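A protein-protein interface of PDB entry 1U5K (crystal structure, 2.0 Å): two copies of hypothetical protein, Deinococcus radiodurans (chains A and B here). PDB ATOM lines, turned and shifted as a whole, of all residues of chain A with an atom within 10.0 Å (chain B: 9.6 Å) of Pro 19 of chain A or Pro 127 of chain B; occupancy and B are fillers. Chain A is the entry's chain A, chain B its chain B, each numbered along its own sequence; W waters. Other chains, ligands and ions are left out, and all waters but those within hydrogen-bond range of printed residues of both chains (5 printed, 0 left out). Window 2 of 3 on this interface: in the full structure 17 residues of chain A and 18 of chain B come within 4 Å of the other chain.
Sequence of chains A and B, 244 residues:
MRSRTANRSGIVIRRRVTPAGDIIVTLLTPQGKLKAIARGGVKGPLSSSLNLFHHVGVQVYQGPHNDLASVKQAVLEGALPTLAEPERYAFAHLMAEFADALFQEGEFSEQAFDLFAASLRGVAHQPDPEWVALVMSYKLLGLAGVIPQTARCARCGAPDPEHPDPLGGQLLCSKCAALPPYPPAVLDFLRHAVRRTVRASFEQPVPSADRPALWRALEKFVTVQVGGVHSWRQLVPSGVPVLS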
ATOM      1  N   ARG A  15     -21.595 -10.125 -31.983  1.00  0.00           N
ATOM      2  CA  ARG A  15     -20.800  -9.239 -32.837  1.00  0.00           C
ATOM      3  C   ARG A  15     -19.418  -9.121 -32.208  1.00  0.00           C
ATOM      4  O   ARG A  15     -19.307  -8.817 -31.019  1.00  0.00           O
ATOM      5  CB  ARG A  15     -21.492  -7.882 -32.941  1.00  0.00           C
ATOM      6  CG  ARG A  15     -20.653  -6.741 -33.469  1.00  0.00           C
ATOM      7  CD  ARG A  15     -21.380  -5.405 -33.462  1.00  0.00           C
ATOM      8  NE  ARG A  15     -20.479  -4.328 -33.874  1.00  0.00           N
ATOM      9  CZ  ARG A  15     -20.545  -3.702 -35.037  1.00  0.00           C
ATOM     10  NH1 ARG A  15     -21.464  -4.036 -35.919  1.00  0.00           N
ATOM     11  NH2 ARG A  15     -19.694  -2.727 -35.324  1.00  0.00           N
ATOM     12  N   ARG A  16     -18.389  -9.475 -32.969  1.00  0.00           N
ATOM     13  CA  ARG A  16     -16.991  -9.264 -32.620  1.00  0.00           C
ATOM     14  C   ARG A  16     -16.364  -8.266 -33.590  1.00  0.00           C
ATOM     15  O   ARG A  16     -16.416  -8.446 -34.805  1.00  0.00           O
ATOM     16  CB  ARG A  16     -16.232 -10.595 -32.648  1.00  0.00           C
ATOM     17  CG  ARG A  16     -14.724 -10.482 -32.427  1.00  0.00           C
ATOM     18  CD  ARG A  16     -14.346 -10.035 -31.015  1.00  0.00           C
ATOM     19  NE  ARG A  16     -14.598 -11.129 -30.083  1.00  0.00           N
ATOM     20  CZ  ARG A  16     -13.769 -12.139 -29.873  1.00  0.00           C
ATOM     21  NH1 ARG A  16     -12.589 -12.188 -30.475  1.00  0.00           N
ATOM     22  NH2 ARG A  16     -14.107 -13.102 -29.024  1.00  0.00           N
ATOM     23  N   VAL A  17     -15.807  -7.193 -33.043  1.00  0.00           N
ATOM     24  CA  VAL A  17     -14.974  -6.253 -33.771  1.00  0.00           C
ATOM     25  C   VAL A  17     -13.550  -6.752 -33.585  1.00  0.00           C
ATOM     26  O   VAL A  17     -12.998  -6.822 -32.491  1.00  0.00           O
ATOM     27  CB  VAL A  17     -15.051  -4.832 -33.214  1.00  0.00           C
ATOM     28  CG1 VAL A  17     -13.944  -3.987 -33.819  1.00  0.00           C
ATOM     29  CG2 VAL A  17     -16.417  -4.203 -33.478  1.00  0.00           C
ATOM     30  N   THR A  18     -12.943  -7.079 -34.712  1.00  0.00           N
ATOM     31  CA  THR A  18     -11.629  -7.698 -34.775  1.00  0.00           C
ATOM     32  C   THR A  18     -10.532  -6.618 -34.760  1.00  0.00           C
ATOM     33  O   THR A  18     -10.813  -5.469 -35.111  1.00  0.00           O
ATOM     34  CB  THR A  18     -11.754  -8.467 -36.103  1.00  0.00           C
ATOM     35  OG1 THR A  18     -11.948  -9.870 -35.864  1.00  0.00           O
ATOM     36  CG2 THR A  18     -10.613  -8.244 -37.037  1.00  0.00           C
ATOM     37  N   PRO A  19      -9.295  -6.927 -34.371  1.00  0.00           N
ATOM     38  CA  PRO A  19      -8.244  -5.897 -34.389  1.00  0.00           C
ATOM     39  C   PRO A  19      -8.052  -5.213 -35.748  1.00  0.00           C
ATOM     40  O   PRO A  19      -7.815  -4.001 -35.787  1.00  0.00           O
ATOM     41  CB  PRO A  19      -6.989  -6.625 -33.896  1.00  0.00           C
ATOM     42  CG  PRO A  19      -7.472  -7.891 -33.277  1.00  0.00           C
ATOM     43  CD  PRO A  19      -8.812  -8.230 -33.876  1.00  0.00           C
ATOM     44  N   ALA A  20      -8.240  -5.951 -36.841  1.00  0.00           N
ATOM     45  CA  ALA A  20      -8.234  -5.402 -38.195  1.00  0.00           C
ATOM     46  C   ALA A  20      -9.447  -4.578 -38.625  1.00  0.00           C
ATOM     47  O   ALA A  20      -9.463  -4.056 -39.741  1.00  0.00           O
ATOM     48  CB  ALA A  20      -8.030  -6.518 -39.209  1.00  0.00           C
ATOM     49  N   GLY A  21     -10.475  -4.464 -37.789  1.00  0.00           N
ATOM     50  CA  GLY A  21     -11.654  -3.703 -38.168  1.00  0.00           C
ATOM     51  C   GLY A  21     -12.684  -4.507 -38.944  1.00  0.00           C
ATOM     52  O   GLY A  21     -13.606  -3.951 -39.543  1.00  0.00           O
ATOM     53  N   ASP A  22     -12.519  -5.824 -38.972  1.00  0.00           N
ATOM     54  CA  ASP A  22     -13.564  -6.706 -39.476  1.00  0.00           C
ATOM     55  C   ASP A  22     -14.654  -6.886 -38.415  1.00  0.00           C
ATOM     56  O   ASP A  22     -14.423  -6.692 -37.218  1.00  0.00           O
ATOM     57  CB  ASP A  22     -12.983  -8.071 -39.853  1.00  0.00           C
ATOM     58  CG  ASP A  22     -11.806  -7.981 -40.819  1.00  0.00           C
ATOM     59  OD1 ASP A  22     -11.815  -7.117 -41.723  1.00  0.00           O
ATOM     60  OD2 ASP A  22     -10.813  -8.741 -40.741  1.00  0.00           O
ATOM     61  N   ILE A  23     -15.846  -7.266 -38.858  1.00  0.00           N
ATOM     62  CA  ILE A  23     -16.951  -7.572 -37.954  1.00  0.00           C
ATOM     63  C   ILE A  23     -17.358  -9.017 -38.177  1.00  0.00           C
ATOM     64  O   ILE A  23     -17.705  -9.382 -39.291  1.00  0.00           O
ATOM     65  CB  ILE A  23     -18.161  -6.655 -38.171  1.00  0.00           C
ATOM     66  CG1 ILE A  23     -17.790  -5.181 -38.060  1.00  0.00           C
ATOM     67  CG2 ILE A  23     -19.256  -6.990 -37.171  1.00  0.00           C
ATOM     68  CD1 ILE A  23     -18.790  -4.278 -38.754  1.00  0.00           C
ATOM     69  N   ILE A  24     -17.220  -9.848 -37.152  1.00  0.00           N
ATOM     70  CA  ILE A  24     -17.590 -11.252 -37.196  1.00  0.00           C
ATOM     71  C   ILE A  24     -18.912 -11.390 -36.441  1.00  0.00           C
ATOM     72  O   ILE A  24     -19.035 -11.012 -35.275  1.00  0.00           O
ATOM     73  CB  ILE A  24     -16.513 -12.122 -36.540  1.00  0.00           C
ATOM     74  CG1 ILE A  24     -15.192 -12.086 -37.314  1.00  0.00           C
ATOM     75  CG2 ILE A  24     -17.019 -13.541 -36.390  1.00  0.00           C
ATOM     76  CD1 ILE A  24     -14.105 -12.932 -36.678  1.00  0.00           C
ATOM     77  N   ILE A  37     -18.182 -13.061 -41.587  1.00  0.00           N
ATOM     78  CA  ILE A  37     -17.301 -11.920 -41.368  1.00  0.00           C
ATOM     79  C   ILE A  37     -17.591 -10.833 -42.398  1.00  0.00           C
ATOM     80  O   ILE A  37     -17.653 -11.132 -43.589  1.00  0.00           O
ATOM     81  CB  ILE A  37     -15.821 -12.356 -41.438  1.00  0.00           C
ATOM     82  CG1 ILE A  37     -14.886 -11.162 -41.225  1.00  0.00           C
ATOM     83  CG2 ILE A  37     -15.455 -13.007 -42.775  1.00  0.00           C
ATOM     84  CD1 ILE A  37     -13.481 -11.592 -40.821  1.00  0.00           C
ATOM     85  N   GLY A  40     -13.359  -5.334 -43.410  1.00  0.00           N
ATOM     86  CA  GLY A  40     -13.306  -3.897 -43.213  1.00  0.00           C
ATOM     87  C   GLY A  40     -14.664  -3.324 -42.865  1.00  0.00           C
ATOM     88  O   GLY A  40     -14.986  -2.199 -43.254  1.00  0.00           O
ATOM     89  N   GLY A  41     -15.449  -4.092 -42.114  1.00  0.00           N
ATOM     90  CA  GLY A  41     -16.843  -3.775 -41.875  1.00  0.00           C
ATOM     91  C   GLY A  41     -17.113  -2.581 -40.980  1.00  0.00           C
ATOM     92  O   GLY A  41     -18.101  -1.876 -41.183  1.00  0.00           O
ATOM     93  N   VAL A  42     -16.269  -2.352 -39.978  1.00  0.00           N
ATOM     94  CA  VAL A  42     -16.513  -1.257 -39.042  1.00  0.00           C
ATOM     95  C   VAL A  42     -16.492   0.091 -39.762  1.00  0.00           C
ATOM     96  O   VAL A  42     -17.314   0.965 -39.480  1.00  0.00           O
ATOM     97  CB  VAL A  42     -15.540  -1.269 -37.844  1.00  0.00           C
ATOM     98  CG1 VAL A  42     -14.132  -0.857 -38.251  1.00  0.00           C
ATOM     99  CG2 VAL A  42     -16.065  -0.366 -36.735  1.00  0.00           C
ATOM    100  N   THR B  82     -20.523  -9.108 -21.220  1.00  0.00           N
ATOM    101  CA  THR B  82     -19.927  -9.749 -22.393  1.00  0.00           C
ATOM    102  C   THR B  82     -19.038 -10.930 -22.053  1.00  0.00           C
ATOM    103  O   THR B  82     -18.609 -11.666 -22.948  1.00  0.00           O
ATOM    104  CB  THR B  82     -19.102  -8.763 -23.228  1.00  0.00           C
ATOM    105  OG1 THR B  82     -18.014  -8.286 -22.431  1.00  0.00           O
ATOM    106  CG2 THR B  82     -19.918  -7.510 -23.602  1.00  0.00           C
ATOM    107  N   GLU B  85     -20.063 -14.343 -23.469  1.00  0.00           N
ATOM    108  CA  GLU B  85     -19.632 -14.824 -24.771  1.00  0.00           C
ATOM    109  C   GLU B  85     -18.618 -15.921 -24.503  1.00  0.00           C
ATOM    110  O   GLU B  85     -17.687 -15.689 -23.729  1.00  0.00           O
ATOM    111  CB  GLU B  85     -19.008 -13.704 -25.603  1.00  0.00           C
ATOM    112  CG  GLU B  85     -19.896 -12.487 -25.810  1.00  0.00           C
ATOM    113  CD  GLU B  85     -19.238 -11.387 -26.625  1.00  0.00           C
ATOM    114  OE1 GLU B  85     -18.131 -11.601 -27.174  1.00  0.00           O
ATOM    115  OE2 GLU B  85     -19.882 -10.328 -26.747  1.00  0.00           O
ATOM    116  N   GLU B  87     -15.947 -17.382 -25.761  1.00  0.00           N
ATOM    117  CA  GLU B  87     -14.508 -17.166 -25.842  1.00  0.00           C
ATOM    118  C   GLU B  87     -14.022 -16.232 -24.745  1.00  0.00           C
ATOM    119  O   GLU B  87     -12.941 -16.412 -24.188  1.00  0.00           O
ATOM    120  CB  GLU B  87     -14.098 -16.576 -27.194  1.00  0.00           C
ATOM    121  CG  GLU B  87     -12.587 -16.400 -27.245  1.00  0.00           C
ATOM    122  CD  GLU B  87     -12.007 -16.054 -28.607  1.00  0.00           C
ATOM    123  OE1 GLU B  87     -12.703 -15.385 -29.397  1.00  0.00           O
ATOM    124  OE2 GLU B  87     -10.866 -16.485 -28.893  1.00  0.00           O
ATOM    125  N   ARG B  88     -14.795 -15.191 -24.475  1.00  0.00           N
ATOM    126  CA  ARG B  88     -14.410 -14.264 -23.426  1.00  0.00           C
ATOM    127  C   ARG B  88     -14.529 -14.927 -22.052  1.00  0.00           C
ATOM    128  O   ARG B  88     -13.671 -14.734 -21.185  1.00  0.00           O
ATOM    129  CB  ARG B  88     -15.222 -12.981 -23.540  1.00  0.00           C
ATOM    130  CG  ARG B  88     -15.003 -12.194 -24.813  1.00  0.00           C
ATOM    131  CD  ARG B  88     -15.827 -10.927 -24.782  1.00  0.00           C
ATOM    132  NE  ARG B  88     -15.821 -10.207 -26.050  1.00  0.00           N
ATOM    133  CZ  ARG B  88     -14.837  -9.450 -26.504  1.00  0.00           C
ATOM    134  NH1 ARG B  88     -15.008  -8.854 -27.672  1.00  0.00           N
ATOM    135  NH2 ARG B  88     -13.700  -9.313 -25.832  1.00  0.00           N
ATOM    136  N   PHE B  91     -11.354 -17.146 -21.379  1.00  0.00           N
ATOM    137  CA  PHE B  91     -10.190 -16.386 -20.934  1.00  0.00           C
ATOM    138  C   PHE B  91     -10.350 -15.820 -19.522  1.00  0.00           C
ATOM    139  O   PHE B  91      -9.412 -15.846 -18.720  1.00  0.00           O
ATOM    140  CB  PHE B  91      -9.816 -15.322 -21.961  1.00  0.00           C
ATOM    141  CG  PHE B  91      -9.104 -15.892 -23.143  1.00  0.00           C
ATOM    142  CD1 PHE B  91      -9.647 -15.864 -24.408  1.00  0.00           C
ATOM    143  CD2 PHE B  91      -7.879 -16.524 -22.972  1.00  0.00           C
ATOM    144  CE1 PHE B  91      -8.981 -16.438 -25.480  1.00  0.00           C
ATOM    145  CE2 PHE B  91      -7.219 -17.095 -24.043  1.00  0.00           C
ATOM    146  CZ  PHE B  91      -7.772 -17.076 -25.293  1.00  0.00           C
ATOM    147  N   ARG B 121     -11.791  -6.772 -17.342  1.00  0.00           N
ATOM    148  CA  ARG B 121     -12.341  -5.724 -18.191  1.00  0.00           C
ATOM    149  C   ARG B 121     -11.801  -5.871 -19.608  1.00  0.00           C
ATOM    150  O   ARG B 121     -12.550  -5.757 -20.574  1.00  0.00           O
ATOM    151  CB  ARG B 121     -12.019  -4.329 -17.662  1.00  0.00           C
ATOM    152  CG  ARG B 121     -12.714  -3.944 -16.377  1.00  0.00           C
ATOM    153  CD  ARG B 121     -12.758  -2.445 -16.171  1.00  0.00           C
ATOM    154  NE  ARG B 121     -11.427  -1.849 -16.098  1.00  0.00           N
ATOM    155  CZ  ARG B 121     -10.597  -1.890 -15.058  1.00  0.00           C
ATOM    156  NH1 ARG B 121     -10.912  -2.546 -13.961  1.00  0.00           N
ATOM    157  NH2 ARG B 121      -9.446  -1.235 -15.082  1.00  0.00           N
ATOM    158  N   GLY B 122     -10.504  -6.132 -19.727  1.00  0.00           N
ATOM    159  CA  GLY B 122      -9.896  -6.275 -21.031  1.00  0.00           C
ATOM    160  C   GLY B 122     -10.414  -7.474 -21.802  1.00  0.00           C
ATOM    161  O   GLY B 122     -10.750  -7.363 -22.988  1.00  0.00           O
ATOM    162  N   VAL B 123     -10.453  -8.625 -21.132  1.00  0.00           N
ATOM    163  CA  VAL B 123     -11.085  -9.804 -21.709  1.00  0.00           C
ATOM    164  C   VAL B 123     -12.516  -9.530 -22.162  1.00  0.00           C
ATOM    165  O   VAL B 123     -12.963  -9.992 -23.218  1.00  0.00           O
ATOM    166  CB  VAL B 123     -10.975 -10.980 -20.736  1.00  0.00           C
ATOM    167  CG1 VAL B 123     -11.902 -12.107 -21.148  1.00  0.00           C
ATOM    168  CG2 VAL B 123      -9.528 -11.455 -20.699  1.00  0.00           C
ATOM    169  N   ALA B 124     -13.237  -8.765 -21.355  1.00  0.00           N
ATOM    170  CA  ALA B 124     -14.622  -8.420 -21.666  1.00  0.00           C
ATOM    171  C   ALA B 124     -14.782  -7.510 -22.870  1.00  0.00           C
ATOM    172  O   ALA B 124     -15.715  -7.700 -23.657  1.00  0.00           O
ATOM    173  CB  ALA B 124     -15.279  -7.765 -20.494  1.00  0.00           C
ATOM    174  N   HIS B 125     -13.875  -6.551 -23.025  1.00  0.00           N
ATOM    175  CA  HIS B 125     -14.109  -5.417 -23.905  1.00  0.00           C
ATOM    176  C   HIS B 125     -13.241  -5.297 -25.150  1.00  0.00           C
ATOM    177  O   HIS B 125     -13.668  -4.728 -26.142  1.00  0.00           O
ATOM    178  CB  HIS B 125     -13.938  -4.111 -23.158  1.00  0.00           C
ATOM    179  CG  HIS B 125     -14.863  -3.942 -22.002  1.00  0.00           C
ATOM    180  ND1 HIS B 125     -16.228  -4.048 -22.117  1.00  0.00           N
ATOM    181  CD2 HIS B 125     -14.609  -3.621 -20.712  1.00  0.00           C
ATOM    182  CE1 HIS B 125     -16.777  -3.828 -20.936  1.00  0.00           C
ATOM    183  NE2 HIS B 125     -15.818  -3.537 -20.076  1.00  0.00           N
ATOM    184  N   GLN B 126     -12.056  -5.884 -25.126  1.00  0.00           N
ATOM    185  CA  GLN B 126     -11.103  -5.731 -26.199  1.00  0.00           C
ATOM    186  C   GLN B 126     -11.290  -6.746 -27.318  1.00  0.00           C
ATOM    187  O   GLN B 126     -11.830  -7.834 -27.114  1.00  0.00           O
ATOM    188  CB  GLN B 126      -9.693  -5.885 -25.635  1.00  0.00           C
ATOM    189  CG  GLN B 126      -9.273  -4.839 -24.645  1.00  0.00           C
ATOM    190  CD  GLN B 126      -9.178  -3.426 -25.186  1.00  0.00           C
ATOM    191  OE1 GLN B 126      -9.898  -3.027 -26.098  1.00  0.00           O
ATOM    192  NE2 GLN B 126      -8.294  -2.651 -24.584  1.00  0.00           N
ATOM    193  N   PRO B 127     -10.896  -6.358 -28.523  1.00  0.00           N
ATOM    194  CA  PRO B 127     -10.952  -7.270 -29.671  1.00  0.00           C
ATOM    195  C   PRO B 127     -10.052  -8.500 -29.572  1.00  0.00           C
ATOM    196  O   PRO B 127     -10.321  -9.466 -30.269  1.00  0.00           O
ATOM    197  CB  PRO B 127     -10.595  -6.370 -30.864  1.00  0.00           C
ATOM    198  CG  PRO B 127      -9.984  -5.167 -30.330  1.00  0.00           C
ATOM    199  CD  PRO B 127     -10.559  -4.986 -28.932  1.00  0.00           C
ATOM    200  N   ASP B 128      -9.010  -8.504 -28.746  1.00  0.00           N
ATOM    201  CA  ASP B 128      -8.084  -9.640 -28.707  1.00  0.00           C
ATOM    202  C   ASP B 128      -7.926 -10.129 -27.264  1.00  0.00           C
ATOM    203  O   ASP B 128      -6.919  -9.846 -26.606  1.00  0.00           O
ATOM    204  CB  ASP B 128      -6.756  -9.195 -29.325  1.00  0.00           C
ATOM    205  CG  ASP B 128      -5.797 -10.338 -29.611  1.00  0.00           C
ATOM    206  OD1 ASP B 128      -5.944 -11.503 -29.156  1.00  0.00           O
ATOM    207  OD2 ASP B 128      -4.837 -10.098 -30.369  1.00  0.00           O
ATOM    208  N   PRO B 129      -8.930 -10.843 -26.759  1.00  0.00           N
ATOM    209  CA  PRO B 129      -8.868 -11.383 -25.399  1.00  0.00           C
ATOM    210  C   PRO B 129      -7.698 -12.309 -25.080  1.00  0.00           C
ATOM    211  O   PRO B 129      -7.257 -12.281 -23.926  1.00  0.00           O
ATOM    212  CB  PRO B 129     -10.193 -12.127 -25.248  1.00  0.00           C
ATOM    213  CG  PRO B 129     -10.656 -12.360 -26.655  1.00  0.00           C
ATOM    214  CD  PRO B 129     -10.237 -11.115 -27.383  1.00  0.00           C
ATOM    215  N   GLU B 130      -7.283 -13.124 -26.048  1.00  0.00           N
ATOM    216  CA  GLU B 130      -6.121 -13.985 -25.898  1.00  0.00           C
ATOM    217  C   GLU B 130      -4.907 -13.132 -25.541  1.00  0.00           C
ATOM    218  O   GLU B 130      -4.215 -13.444 -24.576  1.00  0.00           O
ATOM    219  CB  GLU B 130      -5.812 -14.819 -27.140  1.00  0.00           C
ATOM    220  CG  GLU B 130      -4.620 -15.742 -26.918  1.00  0.00           C
ATOM    221  CD  GLU B 130      -4.107 -16.445 -28.156  1.00  0.00           C
ATOM    222  OE1 GLU B 130      -4.352 -15.927 -29.261  1.00  0.00           O
ATOM    223  OE2 GLU B 130      -3.424 -17.483 -28.005  1.00  0.00           O
ATOM    224  N   TRP B 131      -4.709 -12.044 -26.285  1.00  0.00           N
ATOM    225  CA  TRP B 131      -3.651 -11.096 -26.013  1.00  0.00           C
ATOM    226  C   TRP B 131      -3.755 -10.461 -24.628  1.00  0.00           C
ATOM    227  O   TRP B 131      -2.740 -10.386 -23.939  1.00  0.00           O
ATOM    228  CB  TRP B 131      -3.498 -10.073 -27.135  1.00  0.00           C
ATOM    229  CG  TRP B 131      -2.262  -9.274 -26.999  1.00  0.00           C
ATOM    230  CD1 TRP B 131      -2.167  -7.927 -26.818  1.00  0.00           C
ATOM    231  CD2 TRP B 131      -0.932  -9.782 -26.953  1.00  0.00           C
ATOM    232  NE1 TRP B 131      -0.851  -7.567 -26.655  1.00  0.00           N
ATOM    233  CE2 TRP B 131      -0.073  -8.687 -26.745  1.00  0.00           C
ATOM    234  CE3 TRP B 131      -0.378 -11.062 -27.061  1.00  0.00           C
ATOM    235  CZ2 TRP B 131       1.308  -8.827 -26.633  1.00  0.00           C
ATOM    236  CZ3 TRP B 131       0.995 -11.195 -26.936  1.00  0.00           C
ATOM    237  CH2 TRP B 131       1.812 -10.088 -26.716  1.00  0.00           C
ATOM    238  N   VAL B 132      -4.940 -10.028 -24.197  1.00  0.00           N
ATOM    239  CA  VAL B 132      -5.112  -9.500 -22.852  1.00  0.00           C
ATOM    240  C   VAL B 132      -4.657 -10.532 -21.828  1.00  0.00           C
ATOM    241  O   VAL B 132      -3.945 -10.200 -20.893  1.00  0.00           O
ATOM    242  CB  VAL B 132      -6.567  -9.088 -22.572  1.00  0.00           C
ATOM    243  CG1 VAL B 132      -6.758  -8.584 -21.143  1.00  0.00           C
ATOM    244  CG2 VAL B 132      -6.996  -8.013 -23.545  1.00  0.00           C
ATOM    245  N   PHE B 202      -0.414  -3.700 -24.901  1.00  0.00           N
ATOM    246  CA  PHE B 202      -1.634  -3.861 -25.692  1.00  0.00           C
ATOM    247  C   PHE B 202      -1.388  -3.319 -27.090  1.00  0.00           C
ATOM    248  O   PHE B 202      -1.934  -3.822 -28.063  1.00  0.00           O
ATOM    249  CB  PHE B 202      -2.833  -3.156 -25.036  1.00  0.00           C
ATOM    250  CG  PHE B 202      -3.470  -3.911 -23.900  1.00  0.00           C
ATOM    251  CD1 PHE B 202      -4.572  -3.386 -23.239  1.00  0.00           C
ATOM    252  CD2 PHE B 202      -3.004  -5.147 -23.484  1.00  0.00           C
ATOM    253  CE1 PHE B 202      -5.173  -4.067 -22.193  1.00  0.00           C
ATOM    254  CE2 PHE B 202      -3.587  -5.817 -22.420  1.00  0.00           C
ATOM    255  CZ  PHE B 202      -4.690  -5.305 -21.775  1.00  0.00           C
ATOM    256  N   PRO B 205       0.860  -6.179 -30.017  1.00  0.00           N
ATOM    257  CA  PRO B 205       0.506  -7.599 -30.023  1.00  0.00           C
ATOM    258  C   PRO B 205       1.474  -8.461 -30.830  1.00  0.00           C
ATOM    259  O   PRO B 205       1.934  -8.078 -31.910  1.00  0.00           O
ATOM    260  CB  PRO B 205      -0.874  -7.626 -30.674  1.00  0.00           C
ATOM    261  CG  PRO B 205      -0.985  -6.329 -31.399  1.00  0.00           C
ATOM    262  CD  PRO B 205      -0.218  -5.342 -30.574  1.00  0.00           C
ATOM    263  N   VAL B 206       1.770  -9.640 -30.294  1.00  0.00           N
ATOM    264  CA  VAL B 206       2.635 -10.594 -30.964  1.00  0.00           C
ATOM    265  C   VAL B 206       1.679 -11.289 -31.919  1.00  0.00           C
ATOM    266  O   VAL B 206       0.553 -11.588 -31.526  1.00  0.00           O
ATOM    267  CB  VAL B 206       3.243 -11.581 -29.949  1.00  0.00           C
ATOM    268  CG1 VAL B 206       3.772 -12.831 -30.602  1.00  0.00           C
ATOM    269  CG2 VAL B 206       4.323 -10.913 -29.133  1.00  0.00           C
ATOM    270  N   SER B 208      -0.248 -14.182 -34.051  1.00  0.00           N
ATOM    271  CA  SER B 208      -0.828 -15.368 -33.448  1.00  0.00           C
ATOM    272  C   SER B 208      -0.049 -16.652 -33.705  1.00  0.00           C
ATOM    273  O   SER B 208      -0.119 -17.580 -32.896  1.00  0.00           O
ATOM    274  CB  SER B 208      -2.301 -15.505 -33.838  1.00  0.00           C
ATOM    275  OG  SER B 208      -2.406 -15.922 -35.182  1.00  0.00           O
ATOM    276  N   ARG B 211       2.270 -17.047 -30.728  1.00  0.00           N
ATOM    277  CA  ARG B 211       1.696 -17.139 -29.392  1.00  0.00           C
ATOM    278  C   ARG B 211       1.832 -18.473 -28.684  1.00  0.00           C
ATOM    279  O   ARG B 211       1.919 -18.479 -27.458  1.00  0.00           O
ATOM    280  CB  ARG B 211       0.229 -16.713 -29.408  1.00  0.00           C
ATOM    281  CG  ARG B 211       0.100 -15.224 -29.623  1.00  0.00           C
ATOM    282  CD  ARG B 211      -1.327 -14.759 -29.758  1.00  0.00           C
ATOM    283  NE  ARG B 211      -1.361 -13.370 -30.176  1.00  0.00           N
ATOM    284  CZ  ARG B 211      -2.444 -12.599 -30.180  1.00  0.00           C
ATOM    285  NH1 ARG B 211      -3.624 -13.059 -29.788  1.00  0.00           N
ATOM    286  NH2 ARG B 211      -2.317 -11.334 -30.540  1.00  0.00           N
HETATM  287  O   HOH W   1     -14.283  -6.642 -29.797  1.00  0.00           O
HETATM  288  O   HOH W   2     -16.781 -13.332 -28.434  1.00  0.00           O
HETATM  289  O   HOH W   3     -17.368 -10.098 -29.240  1.00  0.00           O
HETATM  290  O   HOH W   4     -10.477 -13.813 -30.220  1.00  0.00           O
HETATM  291  O   HOH W   5     -21.765  -9.144 -29.171  1.00  0.00           O
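No position is printed for both chains.
Of the 6 pairs that touch across the chains among the printed residues, none has its exchanged pair printed and touching as well.
O of Ile 24 of chain A sits at hydrogen-bond distance from N of Arg 16 of chain A, 2.8 Å away.
The side-chain carboxylate of Glu 85 of chain B lies within salt-bridge range of the guanidinium group of Arg 88 of chain B, 2.9 Å away.
The guanidinium group (NH2) of Arg 88 of chain B lies within hydrogen-bond range of the backbone carbonyl oxygen (O) of Val 123 of chain B (2.8 Å).
The backbone carbonyl oxygen (O) of Ala 124 of chain B lies within hydrogen-bond range of the guanidinium group (NH2) of Arg 88 of chain B.
O of Gln 126 of chain B is in hydrogen-bond range of NH2 of Arg 88 of chain B.
The guanidinium group (NH2) of Arg 16 of chain A is in salt-bridge range of the side-chain carboxylate (OE1) of Glu 87 of chain B (2.7 Å).
The guanidinium group of Arg 16 of chain A sits close to the guanidinium group of Arg 88 of chain B.
Among the printed residues, pairs that only touch across the chains: Val 17 of chain A with Pro 127 of chain B (2.9 Å), Arg 16 of chain A with Pro 127 of chain B (3.5 Å), Pro 19 of chain A with Pro 127 of chain B (3.8 Å) and Thr 18 of chain A with Pro 127 of chain B (3.9 Å).
Of chain B, only Pro 127 comes within 4 Å of Pro 19 of chain A.
Of the printed residues of chain A, Pro 127 of chain B touches Arg 16, Val 17, Thr 18 and Pro 19.
Of chain B, only Pro 127 (3.9 Å) comes within 4 Å of Thr 18 of chain A.
No residue of chain A comes within 4 Å of Asp 128 of chain B.
Printed residues of chain A within 4 Å of Arg 88 of chain B: Arg 16.
Printed residues of chain A within 4 Å of Glu 87 of chain B: Arg 16.
Printed residues of chain B within 4 Å of Arg 16 of chain A: Glu 87 (2.7 Å), Arg 88 (3.3 Å) and Pro 127 (3.5 Å).
Of the printed residues of chain B, Val 17 of chain A touches Pro 127 (2.9 Å).
Arg 121 of chain B touches none of the printed residues of chain A.
The nearest printed residue of chain A that does not touch Arg 88 of chain B is Arg 15 of chain A (5.4 Å).
Printed residues of chain A that touch a printed residue of chain B: Arg 16, Val 17, Thr 18 and Pro 19.
Hydrophobic or aromatic side chains of chain A within 4 Å of the printed part of chain B: Pro 19.
Hydrophobic or aromatic side chains of chain B within 4 Å of the printed part of chain A: Pro 127.
Among the printed residues, 6 pairs touch across the chains.
Among the printed residues, Asp or Glu carboxylates within 4 Å of a Lys or Arg side-chain nitrogen of the other chain: Arg 16 of chain A with Glu 87 of chain B (2.7 Å).
Water W2 bridges the side-chain carboxylate of Glu 85 of chain B and the guanidinium group of Arg 16 of chain A.
Water W3 lies within hydrogen-bond range of the side-chain carboxylate of Glu 85 of chain B (2.7 Å), the backbone carbonyl oxygen of Arg 15 of chain A (2.9 Å), the guanidinium group of Arg 16 of chain A (3.1 Å) and the guanidinium group of Arg 88 of chain B (3.1 Å).
Water W4 bridges NH1 of Arg 16 of chain A (2.7 Å) and OE1 of Glu 87 of chain B (2.8 Å).
Water W5 lies within hydrogen-bond range of the backbone NH of Arg 15 of chain A and the side-chain carboxylate of Glu 85 of chain B.
Water W1 bridges the backbone carbonyl oxygen of Val 17 of chain A and the guanidinium group of Arg 88 of chain B.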
